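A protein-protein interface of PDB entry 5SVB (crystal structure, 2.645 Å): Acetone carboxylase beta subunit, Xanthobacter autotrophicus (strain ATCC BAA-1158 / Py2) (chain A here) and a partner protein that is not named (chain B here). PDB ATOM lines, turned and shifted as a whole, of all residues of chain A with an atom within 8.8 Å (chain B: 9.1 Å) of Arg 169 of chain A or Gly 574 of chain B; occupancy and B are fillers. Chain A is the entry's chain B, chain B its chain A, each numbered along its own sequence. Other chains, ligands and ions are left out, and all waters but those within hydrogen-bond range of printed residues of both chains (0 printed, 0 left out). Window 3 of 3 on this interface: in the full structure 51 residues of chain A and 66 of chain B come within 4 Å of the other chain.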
ATOM      1  N   ARG A 110     -28.200  19.931   7.674  1.00  0.00           N
ATOM      2  CA  ARG A 110     -29.569  20.356   7.932  1.00  0.00           C
ATOM      3  C   ARG A 110     -30.317  20.529   6.619  1.00  0.00           C
ATOM      4  O   ARG A 110     -29.815  21.149   5.679  1.00  0.00           O
ATOM      5  CB  ARG A 110     -29.566  21.668   8.718  1.00  0.00           C
ATOM      6  CG  ARG A 110     -30.948  22.184   9.097  1.00  0.00           C
ATOM      7  CD  ARG A 110     -31.493  21.490  10.325  1.00  0.00           C
ATOM      8  NE  ARG A 110     -30.713  21.814  11.515  1.00  0.00           N
ATOM      9  CZ  ARG A 110     -30.920  22.871  12.293  1.00  0.00           C
ATOM     10  NH1 ARG A 110     -31.892  23.728  12.021  1.00  0.00           N
ATOM     11  NH2 ARG A 110     -30.149  23.073  13.352  1.00  0.00           N
ATOM     12  N   GLY A 153     -29.169  17.232  11.922  1.00  0.00           N
ATOM     13  CA  GLY A 153     -28.528  18.012  10.881  1.00  0.00           C
ATOM     14  C   GLY A 153     -27.862  19.251  11.437  1.00  0.00           C
ATOM     15  O   GLY A 153     -28.307  19.833  12.429  1.00  0.00           O
ATOM     16  N   VAL A 154     -26.778  19.654  10.775  1.00  0.00           N
ATOM     17  CA  VAL A 154     -26.062  20.880  11.096  1.00  0.00           C
ATOM     18  C   VAL A 154     -26.148  21.815   9.898  1.00  0.00           C
ATOM     19  O   VAL A 154     -26.187  21.377   8.743  1.00  0.00           O
ATOM     20  CB  VAL A 154     -24.589  20.612  11.478  1.00  0.00           C
ATOM     21  CG1 VAL A 154     -24.521  19.706  12.691  1.00  0.00           C
ATOM     22  CG2 VAL A 154     -23.824  20.001  10.315  1.00  0.00           C
ATOM     23  N   VAL A 155     -26.183  23.114  10.179  1.00  0.00           N
ATOM     24  CA  VAL A 155     -26.305  24.122   9.133  1.00  0.00           C
ATOM     25  C   VAL A 155     -24.910  24.412   8.590  1.00  0.00           C
ATOM     26  O   VAL A 155     -24.093  25.049   9.256  1.00  0.00           O
ATOM     27  CB  VAL A 155     -26.975  25.396   9.654  1.00  0.00           C
ATOM     28  CG1 VAL A 155     -27.097  26.427   8.542  1.00  0.00           C
ATOM     29  CG2 VAL A 155     -28.339  25.068  10.223  1.00  0.00           C
ATOM     30  N   GLU A 156     -24.643  23.947   7.376  1.00  0.00           N
ATOM     31  CA  GLU A 156     -23.352  24.132   6.733  1.00  0.00           C
ATOM     32  C   GLU A 156     -23.468  23.662   5.294  1.00  0.00           C
ATOM     33  O   GLU A 156     -24.247  22.754   4.994  1.00  0.00           O
ATOM     34  CB  GLU A 156     -22.250  23.354   7.461  1.00  0.00           C
ATOM     35  CG  GLU A 156     -20.898  23.349   6.752  1.00  0.00           C
ATOM     36  CD  GLU A 156     -20.762  22.242   5.720  1.00  0.00           C
ATOM     37  OE1 GLU A 156     -21.697  21.431   5.584  1.00  0.00           O
ATOM     38  OE2 GLU A 156     -19.715  22.182   5.044  1.00  0.00           O
ATOM     39  N   ARG A 157     -22.695  24.288   4.413  1.00  0.00           N
ATOM     40  CA  ARG A 157     -22.562  23.779   3.056  1.00  0.00           C
ATOM     41  C   ARG A 157     -21.202  24.145   2.492  1.00  0.00           C
ATOM     42  O   ARG A 157     -20.795  25.308   2.526  1.00  0.00           O
ATOM     43  CB  ARG A 157     -23.675  24.310   2.139  1.00  0.00           C
ATOM     44  CG  ARG A 157     -25.016  23.607   2.295  1.00  0.00           C
ATOM     45  CD  ARG A 157     -24.954  22.098   1.997  1.00  0.00           C
ATOM     46  NE  ARG A 157     -25.136  21.793   0.581  1.00  0.00           N
ATOM     47  CZ  ARG A 157     -24.157  21.547  -0.282  1.00  0.00           C
ATOM     48  NH1 ARG A 157     -22.885  21.562   0.098  1.00  0.00           N
ATOM     49  NH2 ARG A 157     -24.451  21.280  -1.541  1.00  0.00           N
ATOM     50  N   GLN A 164     -16.665  27.270   1.055  1.00  0.00           N
ATOM     51  CA  GLN A 164     -17.656  27.166   2.126  1.00  0.00           C
ATOM     52  C   GLN A 164     -18.758  28.177   1.849  1.00  0.00           C
ATOM     53  O   GLN A 164     -18.686  29.334   2.258  1.00  0.00           O
ATOM     54  CB  GLN A 164     -17.006  27.392   3.486  1.00  0.00           C
ATOM     55  CG  GLN A 164     -16.002  26.314   3.877  1.00  0.00           C
ATOM     56  CD  GLN A 164     -15.389  26.548   5.244  1.00  0.00           C
ATOM     57  OE1 GLN A 164     -15.939  27.279   6.068  1.00  0.00           O
ATOM     58  NE2 GLN A 164     -14.243  25.928   5.493  1.00  0.00           N
ATOM     59  N   VAL A 165     -19.800  27.726   1.150  1.00  0.00           N
ATOM     60  CA  VAL A 165     -20.894  28.618   0.781  1.00  0.00           C
ATOM     61  C   VAL A 165     -21.627  29.096   2.026  1.00  0.00           C
ATOM     62  O   VAL A 165     -21.867  30.296   2.204  1.00  0.00           O
ATOM     63  CB  VAL A 165     -21.855  27.916  -0.194  1.00  0.00           C
ATOM     64  CG1 VAL A 165     -22.877  28.906  -0.722  1.00  0.00           C
ATOM     65  CG2 VAL A 165     -21.092  27.276  -1.342  1.00  0.00           C
ATOM     66  N   ILE A 166     -22.009  28.166   2.894  1.00  0.00           N
ATOM     67  CA  ILE A 166     -22.655  28.474   4.164  1.00  0.00           C
ATOM     68  C   ILE A 166     -21.695  28.050   5.275  1.00  0.00           C
ATOM     69  O   ILE A 166     -21.516  26.846   5.506  1.00  0.00           O
ATOM     70  CB  ILE A 166     -24.010  27.768   4.301  1.00  0.00           C
ATOM     71  CG1 ILE A 166     -24.895  28.085   3.091  1.00  0.00           C
ATOM     72  CG2 ILE A 166     -24.693  28.205   5.589  1.00  0.00           C
ATOM     73  CD1 ILE A 166     -26.223  27.348   3.072  1.00  0.00           C
ATOM     74  N   PRO A 167     -21.042  28.983   5.966  1.00  0.00           N
ATOM     75  CA  PRO A 167     -20.117  28.590   7.032  1.00  0.00           C
ATOM     76  C   PRO A 167     -20.808  27.757   8.099  1.00  0.00           C
ATOM     77  O   PRO A 167     -22.014  27.873   8.327  1.00  0.00           O
ATOM     78  CB  PRO A 167     -19.631  29.929   7.595  1.00  0.00           C
ATOM     79  CG  PRO A 167     -19.799  30.886   6.478  1.00  0.00           C
ATOM     80  CD  PRO A 167     -21.014  30.435   5.727  1.00  0.00           C
ATOM     81  N   LEU A 168     -20.021  26.912   8.759  1.00  0.00           N
ATOM     82  CA  LEU A 168     -20.558  26.037   9.790  1.00  0.00           C
ATOM     83  C   LEU A 168     -21.080  26.852  10.963  1.00  0.00           C
ATOM     84  O   LEU A 168     -20.375  27.706  11.507  1.00  0.00           O
ATOM     85  CB  LEU A 168     -19.483  25.061  10.266  1.00  0.00           C
ATOM     86  CG  LEU A 168     -19.857  24.191  11.468  1.00  0.00           C
ATOM     87  CD1 LEU A 168     -21.109  23.373  11.185  1.00  0.00           C
ATOM     88  CD2 LEU A 168     -18.701  23.285  11.839  1.00  0.00           C
ATOM     89  N   ARG A 169     -22.323  26.584  11.346  1.00  0.00           N
ATOM     90  CA  ARG A 169     -22.939  27.194  12.521  1.00  0.00           C
ATOM     91  C   ARG A 169     -22.820  26.187  13.659  1.00  0.00           C
ATOM     92  O   ARG A 169     -23.573  25.212  13.727  1.00  0.00           O
ATOM     93  CB  ARG A 169     -24.384  27.579  12.226  1.00  0.00           C
ATOM     94  CG  ARG A 169     -24.498  28.551  11.069  1.00  0.00           C
ATOM     95  CD  ARG A 169     -25.907  29.059  10.863  1.00  0.00           C
ATOM     96  NE  ARG A 169     -25.941  30.103   9.843  1.00  0.00           N
ATOM     97  CZ  ARG A 169     -27.045  30.714   9.427  1.00  0.00           C
ATOM     98  NH1 ARG A 169     -28.224  30.392   9.940  1.00  0.00           N
ATOM     99  NH2 ARG A 169     -26.969  31.652   8.495  1.00  0.00           N
ATOM    100  N   GLU A 170     -21.858  26.426  14.554  1.00  0.00           N
ATOM    101  CA  GLU A 170     -21.471  25.405  15.521  1.00  0.00           C
ATOM    102  C   GLU A 170     -22.553  25.155  16.563  1.00  0.00           C
ATOM    103  O   GLU A 170     -22.625  24.057  17.125  1.00  0.00           O
ATOM    104  CB  GLU A 170     -20.164  25.806  16.202  1.00  0.00           C
ATOM    105  CG  GLU A 170     -19.008  25.984  15.239  1.00  0.00           C
ATOM    106  CD  GLU A 170     -17.675  26.108  15.944  1.00  0.00           C
ATOM    107  OE1 GLU A 170     -17.659  26.102  17.191  1.00  0.00           O
ATOM    108  OE2 GLU A 170     -16.642  26.205  15.252  1.00  0.00           O
ATOM    109  N   ASP A 171     -23.396  26.148  16.844  1.00  0.00           N
ATOM    110  CA  ASP A 171     -24.471  25.935  17.805  1.00  0.00           C
ATOM    111  C   ASP A 171     -25.409  24.826  17.350  1.00  0.00           C
ATOM    112  O   ASP A 171     -25.968  24.106  18.185  1.00  0.00           O
ATOM    113  CB  ASP A 171     -25.247  27.234  18.026  1.00  0.00           C
ATOM    114  CG  ASP A 171     -25.893  27.750  16.756  1.00  0.00           C
ATOM    115  OD1 ASP A 171     -25.255  27.666  15.686  1.00  0.00           O
ATOM    116  OD2 ASP A 171     -27.042  28.237  16.826  1.00  0.00           O
ATOM    117  N   THR A 172     -25.593  24.667  16.037  1.00  0.00           N
ATOM    118  CA  THR A 172     -26.433  23.590  15.528  1.00  0.00           C
ATOM    119  C   THR A 172     -25.762  22.231  15.656  1.00  0.00           C
ATOM    120  O   THR A 172     -26.455  21.208  15.661  1.00  0.00           O
ATOM    121  CB  THR A 172     -26.796  23.844  14.062  1.00  0.00           C
ATOM    122  OG1 THR A 172     -25.608  23.854  13.263  1.00  0.00           O
ATOM    123  CG2 THR A 172     -27.514  25.171  13.914  1.00  0.00           C
ATOM    124  N   ALA A 173     -24.433  22.196  15.755  1.00  0.00           N
ATOM    125  CA  ALA A 173     -23.729  20.941  15.985  1.00  0.00           C
ATOM    126  C   ALA A 173     -23.848  20.504  17.440  1.00  0.00           C
ATOM    127  O   ALA A 173     -24.119  19.332  17.722  1.00  0.00           O
ATOM    128  CB  ALA A 173     -22.262  21.082  15.586  1.00  0.00           C
ATOM    129  N   ARG A 174     -23.653  21.432  18.377  1.00  0.00           N
ATOM    130  CA  ARG A 174     -23.806  21.090  19.786  1.00  0.00           C
ATOM    131  C   ARG A 174     -25.204  20.559  20.067  1.00  0.00           C
ATOM    132  O   ARG A 174     -25.366  19.560  20.778  1.00  0.00           O
ATOM    133  CB  ARG A 174     -23.512  22.308  20.660  1.00  0.00           C
ATOM    134  CG  ARG A 174     -22.154  22.927  20.402  1.00  0.00           C
ATOM    135  CD  ARG A 174     -21.431  23.267  21.693  1.00  0.00           C
ATOM    136  NE  ARG A 174     -20.057  23.701  21.431  1.00  0.00           N
ATOM    137  CZ  ARG A 174     -18.964  22.982  21.670  1.00  0.00           C
ATOM    138  NH1 ARG A 174     -17.771  23.486  21.380  1.00  0.00           N
ATOM    139  NH2 ARG A 174     -19.041  21.771  22.206  1.00  0.00           N
ATOM    140  N   ASP A 175     -26.228  21.210  19.512  1.00  0.00           N
ATOM    141  CA  ASP A 175     -27.598  20.752  19.725  1.00  0.00           C
ATOM    142  C   ASP A 175     -27.815  19.377  19.112  1.00  0.00           C
ATOM    143  O   ASP A 175     -28.476  18.520  19.710  1.00  0.00           O
ATOM    144  CB  ASP A 175     -28.584  21.760  19.141  1.00  0.00           C
ATOM    145  CG  ASP A 175     -28.510  23.110  19.824  1.00  0.00           C
ATOM    146  OD1 ASP A 175     -28.260  23.147  21.048  1.00  0.00           O
ATOM    147  OD2 ASP A 175     -28.700  24.134  19.137  1.00  0.00           O
ATOM    148  N   ALA A 176     -27.271  19.146  17.917  1.00  0.00           N
ATOM    149  CA  ALA A 176     -27.404  17.838  17.286  1.00  0.00           C
ATOM    150  C   ALA A 176     -26.740  16.761  18.131  1.00  0.00           C
ATOM    151  O   ALA A 176     -27.321  15.699  18.377  1.00  0.00           O
ATOM    152  CB  ALA A 176     -26.800  17.873  15.883  1.00  0.00           C
ATOM    153  N   LEU A 192     -20.960  15.144   5.994  1.00  0.00           N
ATOM    154  CA  LEU A 192     -21.349  16.372   5.323  1.00  0.00           C
ATOM    155  C   LEU A 192     -20.890  16.324   3.872  1.00  0.00           C
ATOM    156  O   LEU A 192     -19.918  15.644   3.535  1.00  0.00           O
ATOM    157  CB  LEU A 192     -20.752  17.596   6.025  1.00  0.00           C
ATOM    158  CG  LEU A 192     -21.069  17.713   7.517  1.00  0.00           C
ATOM    159  CD1 LEU A 192     -20.407  18.943   8.104  1.00  0.00           C
ATOM    160  CD2 LEU A 192     -22.563  17.750   7.762  1.00  0.00           C
ATOM    161  N   ASN A 201     -15.019  21.561   7.975  1.00  0.00           N
ATOM    162  CA  ASN A 201     -16.257  21.672   8.742  1.00  0.00           C
ATOM    163  C   ASN A 201     -16.632  20.342   9.381  1.00  0.00           C
ATOM    164  O   ASN A 201     -16.976  20.287  10.566  1.00  0.00           O
ATOM    165  CB  ASN A 201     -17.392  22.166   7.845  1.00  0.00           C
ATOM    166  CG  ASN A 201     -17.251  23.627   7.475  1.00  0.00           C
ATOM    167  OD1 ASN A 201     -16.587  24.394   8.169  1.00  0.00           O
ATOM    168  ND2 ASN A 201     -17.885  24.019   6.378  1.00  0.00           N
ATOM    169  N   ARG A 204     -14.629  19.594  12.263  1.00  0.00           N
ATOM    170  CA  ARG A 204     -14.999  20.473  13.365  1.00  0.00           C
ATOM    171  C   ARG A 204     -16.246  19.952  14.070  1.00  0.00           C
ATOM    172  O   ARG A 204     -16.299  19.897  15.303  1.00  0.00           O
ATOM    173  CB  ARG A 204     -15.216  21.894  12.844  1.00  0.00           C
ATOM    174  CG  ARG A 204     -15.687  22.888  13.892  1.00  0.00           C
ATOM    175  CD  ARG A 204     -14.701  23.007  15.038  1.00  0.00           C
ATOM    176  NE  ARG A 204     -15.223  23.847  16.109  1.00  0.00           N
ATOM    177  CZ  ARG A 204     -14.863  23.753  17.383  1.00  0.00           C
ATOM    178  NH1 ARG A 204     -13.975  22.848  17.768  1.00  0.00           N
ATOM    179  NH2 ARG A 204     -15.402  24.565  18.280  1.00  0.00           N
ATOM    180  N   VAL A 205     -17.263  19.562  13.296  1.00  0.00           N
ATOM    181  CA  VAL A 205     -18.434  18.907  13.871  1.00  0.00           C
ATOM    182  C   VAL A 205     -18.016  17.648  14.618  1.00  0.00           C
ATOM    183  O   VAL A 205     -18.540  17.341  15.694  1.00  0.00           O
ATOM    184  CB  VAL A 205     -19.463  18.593  12.769  1.00  0.00           C
ATOM    185  CG1 VAL A 205     -20.657  17.834  13.336  1.00  0.00           C
ATOM    186  CG2 VAL A 205     -19.925  19.874  12.093  1.00  0.00           C
ATOM    187  N   ILE A 208     -16.725  18.695  17.949  1.00  0.00           N
ATOM    188  CA  ILE A 208     -17.796  19.181  18.814  1.00  0.00           C
ATOM    189  C   ILE A 208     -18.578  18.014  19.397  1.00  0.00           C
ATOM    190  O   ILE A 208     -18.946  18.022  20.578  1.00  0.00           O
ATOM    191  CB  ILE A 208     -18.707  20.151  18.037  1.00  0.00           C
ATOM    192  CG1 ILE A 208     -17.954  21.459  17.771  1.00  0.00           C
ATOM    193  CG2 ILE A 208     -20.009  20.411  18.801  1.00  0.00           C
ATOM    194  CD1 ILE A 208     -18.715  22.467  16.927  1.00  0.00           C
ATOM    195  N   LEU B 567     -29.781  36.298  -0.016  1.00  0.00           N
ATOM    196  CA  LEU B 567     -29.303  35.199   0.816  1.00  0.00           C
ATOM    197  C   LEU B 567     -27.829  35.346   1.158  1.00  0.00           C
ATOM    198  O   LEU B 567     -27.395  34.894   2.222  1.00  0.00           O
ATOM    199  CB  LEU B 567     -29.549  33.862   0.118  1.00  0.00           C
ATOM    200  CG  LEU B 567     -30.776  33.084   0.586  1.00  0.00           C
ATOM    201  CD1 LEU B 567     -31.062  31.937  -0.362  1.00  0.00           C
ATOM    202  CD2 LEU B 567     -30.572  32.565   1.996  1.00  0.00           C
ATOM    203  N   LYS B 568     -27.045  35.964   0.274  1.00  0.00           N
ATOM    204  CA  LYS B 568     -25.626  36.148   0.550  1.00  0.00           C
ATOM    205  C   LYS B 568     -25.417  36.857   1.881  1.00  0.00           C
ATOM    206  O   LYS B 568     -24.590  36.441   2.698  1.00  0.00           O
ATOM    207  CB  LYS B 568     -24.973  36.933  -0.586  1.00  0.00           C
ATOM    208  CG  LYS B 568     -23.481  37.134  -0.416  1.00  0.00           C
ATOM    209  CD  LYS B 568     -22.855  37.674  -1.689  1.00  0.00           C
ATOM    210  CE  LYS B 568     -21.350  37.792  -1.560  1.00  0.00           C
ATOM    211  NZ  LYS B 568     -20.670  37.538  -2.859  1.00  0.00           N
ATOM    212  N   GLU B 569     -26.171  37.930   2.121  1.00  0.00           N
ATOM    213  CA  GLU B 569     -26.031  38.670   3.369  1.00  0.00           C
ATOM    214  C   GLU B 569     -26.696  37.941   4.532  1.00  0.00           C
ATOM    215  O   GLU B 569     -26.190  37.976   5.658  1.00  0.00           O
ATOM    216  CB  GLU B 569     -26.612  40.076   3.209  1.00  0.00           C
ATOM    217  CG  GLU B 569     -26.616  40.909   4.487  1.00  0.00           C
ATOM    218  CD  GLU B 569     -25.234  41.073   5.090  1.00  0.00           C
ATOM    219  OE1 GLU B 569     -24.236  40.899   4.358  1.00  0.00           O
ATOM    220  OE2 GLU B 569     -25.144  41.377   6.299  1.00  0.00           O
ATOM    221  N   LEU B 570     -27.830  37.282   4.285  1.00  0.00           N
ATOM    222  CA  LEU B 570     -28.473  36.507   5.342  1.00  0.00           C
ATOM    223  C   LEU B 570     -27.565  35.383   5.821  1.00  0.00           C
ATOM    224  O   LEU B 570     -27.486  35.106   7.023  1.00  0.00           O
ATOM    225  CB  LEU B 570     -29.803  35.945   4.844  1.00  0.00           C
ATOM    226  CG  LEU B 570     -30.858  36.975   4.436  1.00  0.00           C
ATOM    227  CD1 LEU B 570     -32.027  36.287   3.756  1.00  0.00           C
ATOM    228  CD2 LEU B 570     -31.335  37.769   5.638  1.00  0.00           C
ATOM    229  N   ILE B 571     -26.873  34.723   4.892  1.00  0.00           N
ATOM    230  CA  ILE B 571     -25.898  33.706   5.272  1.00  0.00           C
ATOM    231  C   ILE B 571     -24.784  34.334   6.098  1.00  0.00           C
ATOM    232  O   ILE B 571     -24.430  33.846   7.176  1.00  0.00           O
ATOM    233  CB  ILE B 571     -25.347  33.002   4.019  1.00  0.00           C
ATOM    234  CG1 ILE B 571     -26.447  32.173   3.349  1.00  0.00           C
ATOM    235  CG2 ILE B 571     -24.161  32.108   4.368  1.00  0.00           C
ATOM    236  CD1 ILE B 571     -26.083  31.672   1.968  1.00  0.00           C
ATOM    237  N   ALA B 572     -24.219  35.437   5.603  1.00  0.00           N
ATOM    238  CA  ALA B 572     -23.077  36.052   6.270  1.00  0.00           C
ATOM    239  C   ALA B 572     -23.446  36.555   7.659  1.00  0.00           C
ATOM    240  O   ALA B 572     -22.647  36.451   8.596  1.00  0.00           O
ATOM    241  CB  ALA B 572     -22.532  37.193   5.415  1.00  0.00           C
ATOM    242  N   SER B 573     -24.649  37.108   7.812  1.00  0.00           N
ATOM    243  CA  SER B 573     -25.069  37.662   9.092  1.00  0.00           C
ATOM    244  C   SER B 573     -25.566  36.602  10.065  1.00  0.00           C
ATOM    245  O   SER B 573     -25.817  36.928  11.230  1.00  0.00           O
ATOM    246  CB  SER B 573     -26.163  38.711   8.874  1.00  0.00           C
ATOM    247  OG  SER B 573     -27.310  38.142   8.273  1.00  0.00           O
ATOM    248  N   GLY B 574     -25.711  35.355   9.627  1.00  0.00           N
ATOM    249  CA  GLY B 574     -26.173  34.301  10.505  1.00  0.00           C
ATOM    250  C   GLY B 574     -27.669  34.244  10.691  1.00  0.00           C
ATOM    251  O   GLY B 574     -28.138  33.646  11.664  1.00  0.00           O
ATOM    252  N   ALA B 575     -28.438  34.845   9.788  1.00  0.00           N
ATOM    253  CA  ALA B 575     -29.884  34.876   9.913  1.00  0.00           C
ATOM    254  C   ALA B 575     -30.482  33.534   9.502  1.00  0.00           C
ATOM    255  O   ALA B 575     -29.779  32.602   9.104  1.00  0.00           O
ATOM    256  CB  ALA B 575     -30.463  36.009   9.067  1.00  0.00           C
ATOM    257  N   GLU B 576     -31.803  33.435   9.609  1.00  0.00           N
ATOM    258  CA  GLU B 576     -32.506  32.243   9.159  1.00  0.00           C
ATOM    259  C   GLU B 576     -32.377  32.098   7.649  1.00  0.00           C
ATOM    260  O   GLU B 576     -32.628  33.048   6.903  1.00  0.00           O
ATOM    261  CB  GLU B 576     -33.981  32.319   9.554  1.00  0.00           C
ATOM    262  CG  GLU B 576     -34.261  32.015  11.013  1.00  0.00           C
ATOM    263  CD  GLU B 576     -35.741  32.085  11.342  1.00  0.00           C
ATOM    264  OE1 GLU B 576     -36.470  32.829  10.652  1.00  0.00           O
ATOM    265  OE2 GLU B 576     -36.178  31.392  12.283  1.00  0.00           O
ATOM    266  N   ILE B 577     -31.984  30.910   7.198  1.00  0.00           N
ATOM    267  CA  ILE B 577     -31.884  30.624   5.770  1.00  0.00           C
ATOM    268  C   ILE B 577     -32.789  29.441   5.434  1.00  0.00           C
ATOM    269  O   ILE B 577     -32.851  28.476   6.208  1.00  0.00           O
ATOM    270  CB  ILE B 577     -30.433  30.344   5.350  1.00  0.00           C
ATOM    271  CG1 ILE B 577     -29.803  29.290   6.257  1.00  0.00           C
ATOM    272  CG2 ILE B 577     -29.627  31.625   5.381  1.00  0.00           C
ATOM    273  CD1 ILE B 577     -28.455  28.805   5.776  1.00  0.00           C
ATOM    274  N   PRO B 578     -33.507  29.465   4.311  1.00  0.00           N
ATOM    275  CA  PRO B 578     -34.353  28.319   3.957  1.00  0.00           C
ATOM    276  C   PRO B 578     -33.532  27.053   3.765  1.00  0.00           C
ATOM    277  O   PRO B 578     -32.519  27.052   3.063  1.00  0.00           O
ATOM    278  CB  PRO B 578     -35.018  28.767   2.651  1.00  0.00           C
ATOM    279  CG  PRO B 578     -34.960  30.241   2.675  1.00  0.00           C
ATOM    280  CD  PRO B 578     -33.681  30.580   3.366  1.00  0.00           C
ATOM    281  N   LEU B 579     -33.983  25.969   4.393  1.00  0.00           N
ATOM    282  CA  LEU B 579     -33.324  24.675   4.287  1.00  0.00           C
ATOM    283  C   LEU B 579     -34.373  23.573   4.268  1.00  0.00           C
ATOM    284  O   LEU B 579     -35.504  23.751   4.731  1.00  0.00           O
ATOM    285  CB  LEU B 579     -32.349  24.436   5.446  1.00  0.00           C
ATOM    286  CG  LEU B 579     -31.164  25.395   5.572  1.00  0.00           C
ATOM    287  CD1 LEU B 579     -30.392  25.105   6.847  1.00  0.00           C
ATOM    288  CD2 LEU B 579     -30.250  25.296   4.364  1.00  0.00           C
ATOM    289  N   MET B 593     -38.650  34.288   5.898  1.00  0.00           N
ATOM    290  CA  MET B 593     -37.207  34.451   6.024  1.00  0.00           C
ATOM    291  C   MET B 593     -36.636  35.332   4.921  1.00  0.00           C
ATOM    292  O   MET B 593     -35.511  35.817   5.030  1.00  0.00           O
ATOM    293  CB  MET B 593     -36.510  33.088   5.989  1.00  0.00           C
ATOM    294  CG  MET B 593     -37.020  32.094   7.018  1.00  0.00           C
ATOM    295  SD  MET B 593     -36.139  30.360   6.873  1.00  0.00           S
ATOM    296  CE  MET B 593     -37.274  29.343   8.086  1.00  0.00           C
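NH1 of Arg 169 of chain A is in hydrogen-bond range of O of Ala 575 of chain B, at 2.8 Å.
The backbone NH (N) of Arg 157 of chain A lies within hydrogen-bond range of the backbone carbonyl oxygen (O) of Ile 166 of chain A. OG1 of Thr 172 of chain A is in hydrogen-bond range of N of Val 155 of chain A (3.2 Å). The backbone carbonyl oxygen of Leu 570 of chain B sits at hydrogen-bond distance from the side-chain hydroxyl of Ser 573 of chain B, 3.3 Å away. The backbone NH (N) of Val 165 of chain A sits at hydrogen-bond distance from the backbone carbonyl oxygen (O) of Arg 157 of chain A (3.0 Å). N of Arg 110 of chain A lies within hydrogen-bond range of O of Val 154 of chain A (2.7 Å). The backbone carbonyl oxygen of Leu 570 of chain B sits at hydrogen-bond distance from the backbone NH of Ala 575 of chain B (2.9 Å).
Leu 579 of chain B touches Arg 110 of chain A (CD1 to CG, 3.7 Å). CD1 of Ile 577 of chain B touches CG1 of Val 155 of chain A (3.9 Å). Val 155 of chain A touches Leu 579 of chain B (CG1 to CD1, 3.9 Å). O of Val 165 of chain A touches CG2 of Ile 571 of chain B, 3.6 Å away. Ile 166 of chain A touches Ile 571 of chain B (CA to CG2, 3.9 Å). CD1 of Ile 577 of chain B touches CD1 of Ile 166 of chain A, 3.8 Å away. Ile 571 of chain B touches Pro 167 of chain A (CG2 to CD, 3.8 Å). NH2 of Arg 169 of chain A touches O of Leu 570 of chain B, 3.8 Å away. Ile 571 of chain B touches Arg 169 of chain A. Gly 574 of chain B touches Arg 169 of chain A (CA to NH2, 3.4 Å).
Arg 169 of chain A touches four residues of chain B. Gly 574 of chain B touches just one residue of chain A: Arg 169 (3.4 Å). Val 155 of chain A touches just these residues of chain B: Ile 577 and Leu 579. No residue of chain B comes within 4 Å of Leu 168 of chain A. Of chain A, only Arg 169 comes within 4 Å of Ala 575 of chain B. Of the printed residues of chain B, Val 165 of chain A touches Ile 571 (3.6 Å). Printed residues of chain B within 4 Å of Arg 110 of chain A: Leu 579 (3.7 Å). Printed residues of chain A within 4 Å of Ile 577 of chain B: Val 155 and Ile 166. Of the printed residues of chain A, Ile 571 of chain B touches Val 165 (3.6 Å), Ile 166 (3.9 Å), Pro 167 (3.8 Å) and Arg 169 (3.6 Å). Printed residues of chain B within 4 Å of Pro 167 of chain A: Ile 571. The nearest residue of chain A that does not touch Gly 574 of chain B is Asp 171 of chain A (7.6 Å). The nearest printed residue of chain A that does not touch Leu 570 of chain B is Ile 166 of chain A (7.6 Å).
Along chain A the printed residues that touch a printed residue of chain B span positions 110 to 169.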
